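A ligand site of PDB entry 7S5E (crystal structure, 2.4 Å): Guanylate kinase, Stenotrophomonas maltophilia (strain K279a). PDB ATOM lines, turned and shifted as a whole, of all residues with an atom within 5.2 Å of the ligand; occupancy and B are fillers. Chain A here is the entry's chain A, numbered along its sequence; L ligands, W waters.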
ATOM      1  N   ALA A  29     -14.559 -23.738  14.906  1.00  0.00           N
ATOM      2  CA  ALA A  29     -15.797 -23.095  14.488  1.00  0.00           C
ATOM      3  C   ALA A  29     -16.761 -23.122  15.649  1.00  0.00           C
ATOM      4  O   ALA A  29     -16.706 -24.048  16.460  1.00  0.00           O
ATOM      5  CB  ALA A  29     -16.417 -23.781  13.278  1.00  0.00           C
ATOM      6  N   PRO A  30     -17.675 -22.158  15.770  1.00  0.00           N
ATOM      7  CA  PRO A  30     -18.765 -22.325  16.729  1.00  0.00           C
ATOM      8  C   PRO A  30     -19.636 -23.487  16.301  1.00  0.00           C
ATOM      9  O   PRO A  30     -19.736 -23.817  15.126  1.00  0.00           O
ATOM     10  CB  PRO A  30     -19.527 -20.990  16.647  1.00  0.00           C
ATOM     11  CG  PRO A  30     -19.281 -20.527  15.255  1.00  0.00           C
ATOM     12  CD  PRO A  30     -17.866 -20.949  14.939  1.00  0.00           C
ATOM     13  N   SER A  31     -20.257 -24.130  17.285  1.00  0.00           N
ATOM     14  CA  SER A  31     -21.176 -25.217  16.958  1.00  0.00           C
ATOM     15  C   SER A  31     -22.280 -24.690  16.065  1.00  0.00           C
ATOM     16  O   SER A  31     -22.759 -23.559  16.224  1.00  0.00           O
ATOM     17  CB  SER A  31     -21.740 -25.838  18.234  1.00  0.00           C
ATOM     18  OG  SER A  31     -22.480 -24.898  18.969  1.00  0.00           O
ATOM     19  N   LYS A  35     -18.706 -27.444  11.059  1.00  0.00           N
ATOM     20  CA  LYS A  35     -17.336 -27.944  10.949  1.00  0.00           C
ATOM     21  C   LYS A  35     -17.277 -29.471  11.005  1.00  0.00           C
ATOM     22  O   LYS A  35     -16.544 -30.084  10.225  1.00  0.00           O
ATOM     23  CB  LYS A  35     -16.436 -27.296  12.009  1.00  0.00           C
ATOM     24  CG  LYS A  35     -16.473 -27.864  13.414  1.00  0.00           C
ATOM     25  CD  LYS A  35     -15.226 -27.413  14.171  1.00  0.00           C
ATOM     26  CE  LYS A  35     -15.301 -27.699  15.649  1.00  0.00           C
ATOM     27  NZ  LYS A  35     -16.329 -26.836  16.302  1.00  0.00           N
ATOM     28  N   SER A  54     -11.646 -36.268  21.298  1.00  0.00           N
ATOM     29  CA  SER A  54     -11.401 -35.515  22.520  1.00  0.00           C
ATOM     30  C   SER A  54     -12.073 -36.160  23.741  1.00  0.00           C
ATOM     31  O   SER A  54     -13.046 -36.904  23.639  1.00  0.00           O
ATOM     32  CB  SER A  54     -11.927 -34.090  22.367  1.00  0.00           C
ATOM     33  OG  SER A  54     -11.328 -33.416  21.270  1.00  0.00           O
ATOM     34  N   PHE A  55     -11.517 -35.850  24.919  1.00  0.00           N
ATOM     35  CA  PHE A  55     -12.173 -36.125  26.188  1.00  0.00           C
ATOM     36  C   PHE A  55     -13.018 -34.946  26.617  1.00  0.00           C
ATOM     37  O   PHE A  55     -12.677 -33.786  26.367  1.00  0.00           O
ATOM     38  CB  PHE A  55     -11.149 -36.420  27.291  1.00  0.00           C
ATOM     39  CG  PHE A  55     -10.546 -37.781  27.208  1.00  0.00           C
ATOM     40  CD1 PHE A  55      -9.568 -38.071  26.273  1.00  0.00           C
ATOM     41  CD2 PHE A  55     -10.945 -38.775  28.078  1.00  0.00           C
ATOM     42  CE1 PHE A  55      -9.011 -39.316  26.201  1.00  0.00           C
ATOM     43  CE2 PHE A  55     -10.390 -40.042  28.016  1.00  0.00           C
ATOM     44  CZ  PHE A  55      -9.419 -40.311  27.075  1.00  0.00           C
ATOM     45  N   ARG A  58     -18.563 -32.872  29.903  1.00  0.00           N
ATOM     46  CA  ARG A  58     -19.956 -32.511  29.707  1.00  0.00           C
ATOM     47  C   ARG A  58     -20.794 -33.759  29.439  1.00  0.00           C
ATOM     48  O   ARG A  58     -20.293 -34.793  28.974  1.00  0.00           O
ATOM     49  CB  ARG A  58     -20.111 -31.497  28.578  1.00  0.00           C
ATOM     50  CG  ARG A  58     -20.048 -32.081  27.191  1.00  0.00           C
ATOM     51  CD  ARG A  58     -20.998 -31.336  26.281  1.00  0.00           C
ATOM     52  NE  ARG A  58     -20.727 -31.575  24.865  1.00  0.00           N
ATOM     53  CZ  ARG A  58     -21.167 -32.619  24.186  1.00  0.00           C
ATOM     54  NH1 ARG A  58     -21.846 -33.595  24.768  1.00  0.00           N
ATOM     55  NH2 ARG A  58     -20.933 -32.690  22.872  1.00  0.00           N
ATOM     56  N   ARG A  61     -25.148 -35.637  24.717  1.00  0.00           N
ATOM     57  CA  ARG A  61     -26.360 -35.185  24.042  1.00  0.00           C
ATOM     58  C   ARG A  61     -26.969 -36.319  23.224  1.00  0.00           C
ATOM     59  O   ARG A  61     -26.276 -37.263  22.838  1.00  0.00           O
ATOM     60  CB  ARG A  61     -26.048 -33.994  23.154  1.00  0.00           C
ATOM     61  CG  ARG A  61     -25.428 -32.864  23.930  1.00  0.00           C
ATOM     62  CD  ARG A  61     -24.922 -31.776  23.029  1.00  0.00           C
ATOM     63  NE  ARG A  61     -24.293 -30.728  23.818  1.00  0.00           N
ATOM     64  CZ  ARG A  61     -23.478 -29.808  23.318  1.00  0.00           C
ATOM     65  NH1 ARG A  61     -23.172 -29.786  22.036  1.00  0.00           N
ATOM     66  NH2 ARG A  61     -22.951 -28.904  24.134  1.00  0.00           N
ATOM     67  N   GLU A  64     -25.245 -38.750  20.392  1.00  0.00           N
ATOM     68  CA  GLU A  64     -23.833 -38.954  20.645  1.00  0.00           C
ATOM     69  C   GLU A  64     -23.591 -40.343  21.228  1.00  0.00           C
ATOM     70  O   GLU A  64     -24.445 -40.904  21.923  1.00  0.00           O
ATOM     71  CB  GLU A  64     -23.307 -37.872  21.588  1.00  0.00           C
ATOM     72  CG  GLU A  64     -23.049 -36.564  20.864  1.00  0.00           C
ATOM     73  CD  GLU A  64     -22.576 -35.463  21.781  1.00  0.00           C
ATOM     74  OE1 GLU A  64     -23.006 -35.425  22.964  1.00  0.00           O
ATOM     75  OE2 GLU A  64     -21.789 -34.611  21.315  1.00  0.00           O
ATOM     76  N   TYR A  70     -16.844 -38.562  21.427  1.00  0.00           N
ATOM     77  CA  TYR A  70     -16.007 -38.084  22.513  1.00  0.00           C
ATOM     78  C   TYR A  70     -15.690 -39.270  23.411  1.00  0.00           C
ATOM     79  O   TYR A  70     -16.379 -40.292  23.407  1.00  0.00           O
ATOM     80  CB  TYR A  70     -16.732 -37.020  23.328  1.00  0.00           C
ATOM     81  CG  TYR A  70     -16.798 -35.644  22.724  1.00  0.00           C
ATOM     82  CD1 TYR A  70     -17.914 -35.238  22.003  1.00  0.00           C
ATOM     83  CD2 TYR A  70     -15.752 -34.757  22.874  1.00  0.00           C
ATOM     84  CE1 TYR A  70     -17.984 -33.980  21.464  1.00  0.00           C
ATOM     85  CE2 TYR A  70     -15.814 -33.488  22.330  1.00  0.00           C
ATOM     86  CZ  TYR A  70     -16.940 -33.106  21.625  1.00  0.00           C
ATOM     87  OH  TYR A  70     -17.037 -31.850  21.078  1.00  0.00           O
ATOM     88  N   GLU A  89      -3.448 -30.621  25.269  1.00  0.00           N
ATOM     89  CA  GLU A  89      -4.118 -29.377  25.613  1.00  0.00           C
ATOM     90  C   GLU A  89      -5.434 -29.725  26.286  1.00  0.00           C
ATOM     91  O   GLU A  89      -6.006 -30.802  26.062  1.00  0.00           O
ATOM     92  CB  GLU A  89      -4.359 -28.500  24.375  1.00  0.00           C
ATOM     93  CG  GLU A  89      -5.236 -29.122  23.281  1.00  0.00           C
ATOM     94  CD  GLU A  89      -6.731 -29.050  23.586  1.00  0.00           C
ATOM     95  OE1 GLU A  89      -7.163 -28.106  24.272  1.00  0.00           O
ATOM     96  OE2 GLU A  89      -7.476 -29.954  23.125  1.00  0.00           O
ATOM     97  N   HIS A  90      -5.921 -28.800  27.095  1.00  0.00           N
ATOM     98  CA  HIS A  90      -7.255 -28.914  27.655  1.00  0.00           C
ATOM     99  C   HIS A  90      -7.738 -27.512  28.006  1.00  0.00           C
ATOM    100  O   HIS A  90      -6.939 -26.595  28.218  1.00  0.00           O
ATOM    101  CB  HIS A  90      -7.285 -29.826  28.895  1.00  0.00           C
ATOM    102  CG  HIS A  90      -6.680 -29.214  30.121  1.00  0.00           C
ATOM    103  ND1 HIS A  90      -5.337 -29.287  30.411  1.00  0.00           N
ATOM    104  CD2 HIS A  90      -7.248 -28.512  31.136  1.00  0.00           C
ATOM    105  CE1 HIS A  90      -5.096 -28.666  31.546  1.00  0.00           C
ATOM    106  NE2 HIS A  90      -6.240 -28.186  32.010  1.00  0.00           N
ATOM    107  N   ALA A  91      -9.061 -27.368  28.079  1.00  0.00           N
ATOM    108  CA  ALA A  91      -9.630 -26.054  28.336  1.00  0.00           C
ATOM    109  C   ALA A  91     -11.035 -26.225  28.898  1.00  0.00           C
ATOM    110  O   ALA A  91     -11.687 -27.263  28.710  1.00  0.00           O
ATOM    111  CB  ALA A  91      -9.647 -25.175  27.085  1.00  0.00           C
ATOM    112  N   VAL A  93     -14.559 -25.166  28.417  1.00  0.00           N
ATOM    113  CA  VAL A  93     -15.319 -24.757  27.239  1.00  0.00           C
ATOM    114  C   VAL A  93     -16.796 -24.867  27.568  1.00  0.00           C
ATOM    115  O   VAL A  93     -17.301 -25.976  27.765  1.00  0.00           O
ATOM    116  CB  VAL A  93     -14.970 -25.616  26.017  1.00  0.00           C
ATOM    117  CG1 VAL A  93     -15.811 -25.215  24.838  1.00  0.00           C
ATOM    118  CG2 VAL A  93     -13.493 -25.508  25.710  1.00  0.00           C
ATOM    119  N   HIS A  94     -17.501 -23.741  27.591  1.00  0.00           N
ATOM    120  CA  HIS A  94     -18.940 -23.708  27.840  1.00  0.00           C
ATOM    121  C   HIS A  94     -19.304 -24.378  29.171  1.00  0.00           C
ATOM    122  O   HIS A  94     -20.276 -25.132  29.253  1.00  0.00           O
ATOM    123  CB  HIS A  94     -19.699 -24.416  26.707  1.00  0.00           C
ATOM    124  CG  HIS A  94     -19.302 -23.980  25.330  1.00  0.00           C
ATOM    125  ND1 HIS A  94     -18.839 -22.713  25.040  1.00  0.00           N
ATOM    126  CD2 HIS A  94     -19.286 -24.664  24.160  1.00  0.00           C
ATOM    127  CE1 HIS A  94     -18.569 -22.632  23.749  1.00  0.00           C
ATOM    128  NE2 HIS A  94     -18.830 -23.795  23.192  1.00  0.00           N
ATOM    129  N   LYS A  98     -12.884 -29.849  28.195  1.00  0.00           N
ATOM    130  CA  LYS A  98     -12.596 -30.475  26.907  1.00  0.00           C
ATOM    131  C   LYS A  98     -11.089 -30.620  26.810  1.00  0.00           C
ATOM    132  O   LYS A  98     -10.349 -29.759  27.294  1.00  0.00           O
ATOM    133  CB  LYS A  98     -13.111 -29.637  25.708  1.00  0.00           C
ATOM    134  CG  LYS A  98     -14.623 -29.539  25.598  1.00  0.00           C
ATOM    135  CD  LYS A  98     -15.182 -30.727  24.852  1.00  0.00           C
ATOM    136  CE  LYS A  98     -16.700 -30.711  24.832  1.00  0.00           C
ATOM    137  NZ  LYS A  98     -17.284 -29.612  24.034  1.00  0.00           N
ATOM    138  N   GLY A  99     -10.613 -31.711  26.205  1.00  0.00           N
ATOM    139  CA  GLY A  99      -9.182 -31.895  26.125  1.00  0.00           C
ATOM    140  C   GLY A  99      -8.754 -32.946  25.135  1.00  0.00           C
ATOM    141  O   GLY A  99      -9.501 -33.888  24.823  1.00  0.00           O
ATOM    142  N   THR A 100      -7.508 -32.801  24.674  1.00  0.00           N
ATOM    143  CA  THR A 100      -6.867 -33.741  23.764  1.00  0.00           C
ATOM    144  C   THR A 100      -5.796 -34.490  24.536  1.00  0.00           C
ATOM    145  O   THR A 100      -4.867 -33.872  25.082  1.00  0.00           O
ATOM    146  CB  THR A 100      -6.246 -33.004  22.579  1.00  0.00           C
ATOM    147  OG1 THR A 100      -7.233 -32.164  21.961  1.00  0.00           O
ATOM    148  CG2 THR A 100      -5.726 -34.003  21.562  1.00  0.00           C
ATOM    149  N   GLU A 118     -10.075 -30.865  16.457  1.00  0.00           N
ATOM    150  CA  GLU A 118     -11.273 -30.011  16.433  1.00  0.00           C
ATOM    151  C   GLU A 118     -11.414 -29.456  17.840  1.00  0.00           C
ATOM    152  O   GLU A 118     -11.995 -30.093  18.710  1.00  0.00           O
ATOM    153  CB  GLU A 118     -12.543 -30.756  16.028  1.00  0.00           C
ATOM    154  CG  GLU A 118     -12.579 -31.306  14.619  1.00  0.00           C
ATOM    155  CD  GLU A 118     -13.912 -31.966  14.290  1.00  0.00           C
ATOM    156  OE1 GLU A 118     -14.937 -31.538  14.868  1.00  0.00           O
ATOM    157  OE2 GLU A 118     -13.911 -32.950  13.525  1.00  0.00           O
ATOM    158  N   ILE A 119     -10.835 -28.289  18.078  1.00  0.00           N
ATOM    159  CA  ILE A 119     -10.780 -27.698  19.410  1.00  0.00           C
ATOM    160  C   ILE A 119     -11.232 -26.247  19.354  1.00  0.00           C
ATOM    161  O   ILE A 119     -11.458 -25.681  18.285  1.00  0.00           O
ATOM    162  CB  ILE A 119      -9.368 -27.821  20.014  1.00  0.00           C
ATOM    163  CG1 ILE A 119      -8.371 -27.081  19.109  1.00  0.00           C
ATOM    164  CG2 ILE A 119      -8.985 -29.291  20.188  1.00  0.00           C
ATOM    165  CD1 ILE A 119      -6.935 -27.278  19.488  1.00  0.00           C
ATOM    166  N   ASP A 120     -11.392 -25.648  20.533  1.00  0.00           N
ATOM    167  CA  ASP A 120     -11.786 -24.259  20.625  1.00  0.00           C
ATOM    168  C   ASP A 120     -10.545 -23.367  20.525  1.00  0.00           C
ATOM    169  O   ASP A 120      -9.413 -23.846  20.390  1.00  0.00           O
ATOM    170  CB  ASP A 120     -12.556 -23.992  21.924  1.00  0.00           C
ATOM    171  CG  ASP A 120     -11.655 -23.712  23.110  1.00  0.00           C
ATOM    172  OD1 ASP A 120     -10.590 -24.338  23.247  1.00  0.00           O
ATOM    173  OD2 ASP A 120     -12.029 -22.872  23.953  1.00  0.00           O
ATOM    174  N   GLY A 123      -7.790 -23.968  23.285  1.00  0.00           N
ATOM    175  CA  GLY A 123      -6.913 -25.090  23.013  1.00  0.00           C
ATOM    176  C   GLY A 123      -5.972 -24.823  21.858  1.00  0.00           C
ATOM    177  O   GLY A 123      -4.818 -25.256  21.875  1.00  0.00           O
ATOM    178  N   GLU A 172     -16.956 -17.466  20.668  1.00  0.00           N
ATOM    179  CA  GLU A 172     -15.965 -18.221  19.917  1.00  0.00           C
ATOM    180  C   GLU A 172     -15.504 -17.443  18.686  1.00  0.00           C
ATOM    181  O   GLU A 172     -14.305 -17.363  18.410  1.00  0.00           O
ATOM    182  CB  GLU A 172     -16.549 -19.560  19.498  1.00  0.00           C
ATOM    183  CG  GLU A 172     -15.549 -20.422  18.816  1.00  0.00           C
ATOM    184  CD  GLU A 172     -14.861 -21.367  19.759  1.00  0.00           C
ATOM    185  OE1 GLU A 172     -14.991 -21.186  20.998  1.00  0.00           O
ATOM    186  OE2 GLU A 172     -14.146 -22.266  19.260  1.00  0.00           O
HETATM  187  P1  LIG L   1     -19.603 -29.256  21.818  1.00  0.00           P
HETATM  188  O1  LIG L   1     -19.306 -30.695  21.374  1.00  0.00           O
HETATM  189  O2  LIG L   1     -19.697 -29.217  23.350  1.00  0.00           O
HETATM  190  O3  LIG L   1     -20.715 -28.642  21.038  1.00  0.00           O
HETATM  191  O4  LIG L   1     -18.271 -28.466  21.440  1.00  0.00           O
HETATM  192  C1  LIG L   1     -17.979 -27.226  22.054  1.00  0.00           C
HETATM  193  C2  LIG L   1     -16.654 -26.680  21.596  1.00  0.00           C
HETATM  194  O5  LIG L   1     -15.576 -27.448  22.189  1.00  0.00           O
HETATM  195  C3  LIG L   1     -16.429 -26.718  20.069  1.00  0.00           C
HETATM  196  O6  LIG L   1     -15.867 -25.477  19.640  1.00  0.00           O
HETATM  197  C4  LIG L   1     -15.375 -27.805  19.895  1.00  0.00           C
HETATM  198  O7  LIG L   1     -14.536 -27.623  18.781  1.00  0.00           O
HETATM  199  C5  LIG L   1     -14.601 -27.692  21.201  1.00  0.00           C
HETATM  200  N1  LIG L   1     -13.815 -28.881  21.532  1.00  0.00           N
HETATM  201  C6  LIG L   1     -14.012 -30.165  21.115  1.00  0.00           C
HETATM  202  N2  LIG L   1     -13.043 -30.964  21.446  1.00  0.00           N
HETATM  203  C7  LIG L   1     -12.156 -30.166  22.153  1.00  0.00           C
HETATM  204  C8  LIG L   1     -10.881 -30.460  22.733  1.00  0.00           C
HETATM  205  O8  LIG L   1     -10.289 -31.536  22.709  1.00  0.00           O
HETATM  206  N3  LIG L   1     -10.321 -29.356  23.335  1.00  0.00           N
HETATM  207  C9  LIG L   1     -10.892 -28.110  23.381  1.00  0.00           C
HETATM  208  N4  LIG L   1     -10.211 -27.162  24.031  1.00  0.00           N
HETATM  209  N5  LIG L   1     -12.065 -27.820  22.836  1.00  0.00           N
HETATM  210  C10 LIG L   1     -12.635 -28.884  22.230  1.00  0.00           C
HETATM  211  O   HOH W   1     -13.971 -24.876  17.741  1.00  0.00           O
HETATM  212  O   HOH W   2     -12.761 -32.696  19.308  1.00  0.00           O
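O8 of the ligand lies close to O of Gly 99 (3.3 Å). A nitrogen (N2) of the ligand lies close to the backbone carbonyl oxygen of Glu 118, at 3.1 Å. O of Ala 29 touches O6 of the ligand (3.6 Å). Ala 91 touches the ligand (CB to N4, 3.7 Å). Val 93 touches the ligand (CG1 to O5, 3.5 Å). CD2 of His 94 touches C1 of the ligand, 3.6 Å away. CG2 of Ile 119 touches C8 of the ligand, at 3.4 Å. OE2 of Glu 172 touches O6 of the ligand (3.7 Å). Of the 23 residues printed, 17 come within 4 Å of the ligand.
The backbone carbonyl oxygen (O) of Lys 98 sits at hydrogen-bond distance from the backbone NH (N) of Ala 91, 2.8 Å away. OE1 of Glu 64 is in hydrogen-bond range of N of Arg 61, 2.8 Å away. The guanidinium group (NH2) of Arg 58 lies within salt-bridge range of the side-chain carboxylate (OE2) of Glu 64 (2.6 Å). The backbone carbonyl oxygen (O) of Ala 29 lies within hydrogen-bond range of the side-chain amino group (NZ) of Lys 35 (2.8 Å). OE2 of Glu 89 lies within hydrogen-bond range of OG1 of Thr 100 (2.5 Å). OD1 of Asp 120 lies within hydrogen-bond range of N of Gly 123. The backbone carbonyl oxygen of Gly 99 sits at hydrogen-bond distance from the backbone NH of Phe 55.
Water W1 lies within hydrogen-bond range of the backbone carbonyl oxygen (O) of Ile 119 (2.7 Å), an oxygen (O6) of the ligand (2.7 Å), the side-chain carboxylate (OE2) of Glu 172 (3.0 Å), the backbone NH (N) of Ala 29 (3.1 Å) and the side-chain amino group (NZ) of Lys 35 (3.4 Å). Water W2 lies within hydrogen-bond range of OG of Ser 54 (2.5 Å), N2 of the ligand (2.8 Å) and O of Glu 118 (2.8 Å).
The guanidinium group (NH1) of Arg 61 lies within salt-bridge range of an oxygen (O3) of the ligand (2.9 Å). N of Asp 120 sits at hydrogen-bond distance from N5 of the ligand (3.2 Å). OE2 of Glu 89 is in hydrogen-bond range of N3 of the ligand, at 2.9 Å. The side-chain amino group (NZ) of Lys 98 is in salt-bridge range of an oxygen (O2) of the ligand, at 2.5 Å. The guanidinium group of Arg 58 lies within salt-bridge range of an oxygen (O1) of the ligand (3.0 Å). The side-chain amino group (NZ) of Lys 35 lies within hydrogen-bond range of an oxygen (O7) of the ligand (3.2 Å). An oxygen (O8) of the ligand lies within hydrogen-bond range of the side-chain hydroxyl of Thr 100 (3.2 Å). OH of Tyr 70 sits at hydrogen-bond distance from O1 of the ligand, at 2.6 Å. The side-chain hydroxyl (OG) of Ser 54 sits at hydrogen-bond distance from an oxygen (O8) of the ligand (2.6 Å). A nitrogen (N4) of the ligand sits at hydrogen-bond distance from the side-chain carboxylate (OD1) of Asp 120, at 3.0 Å.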
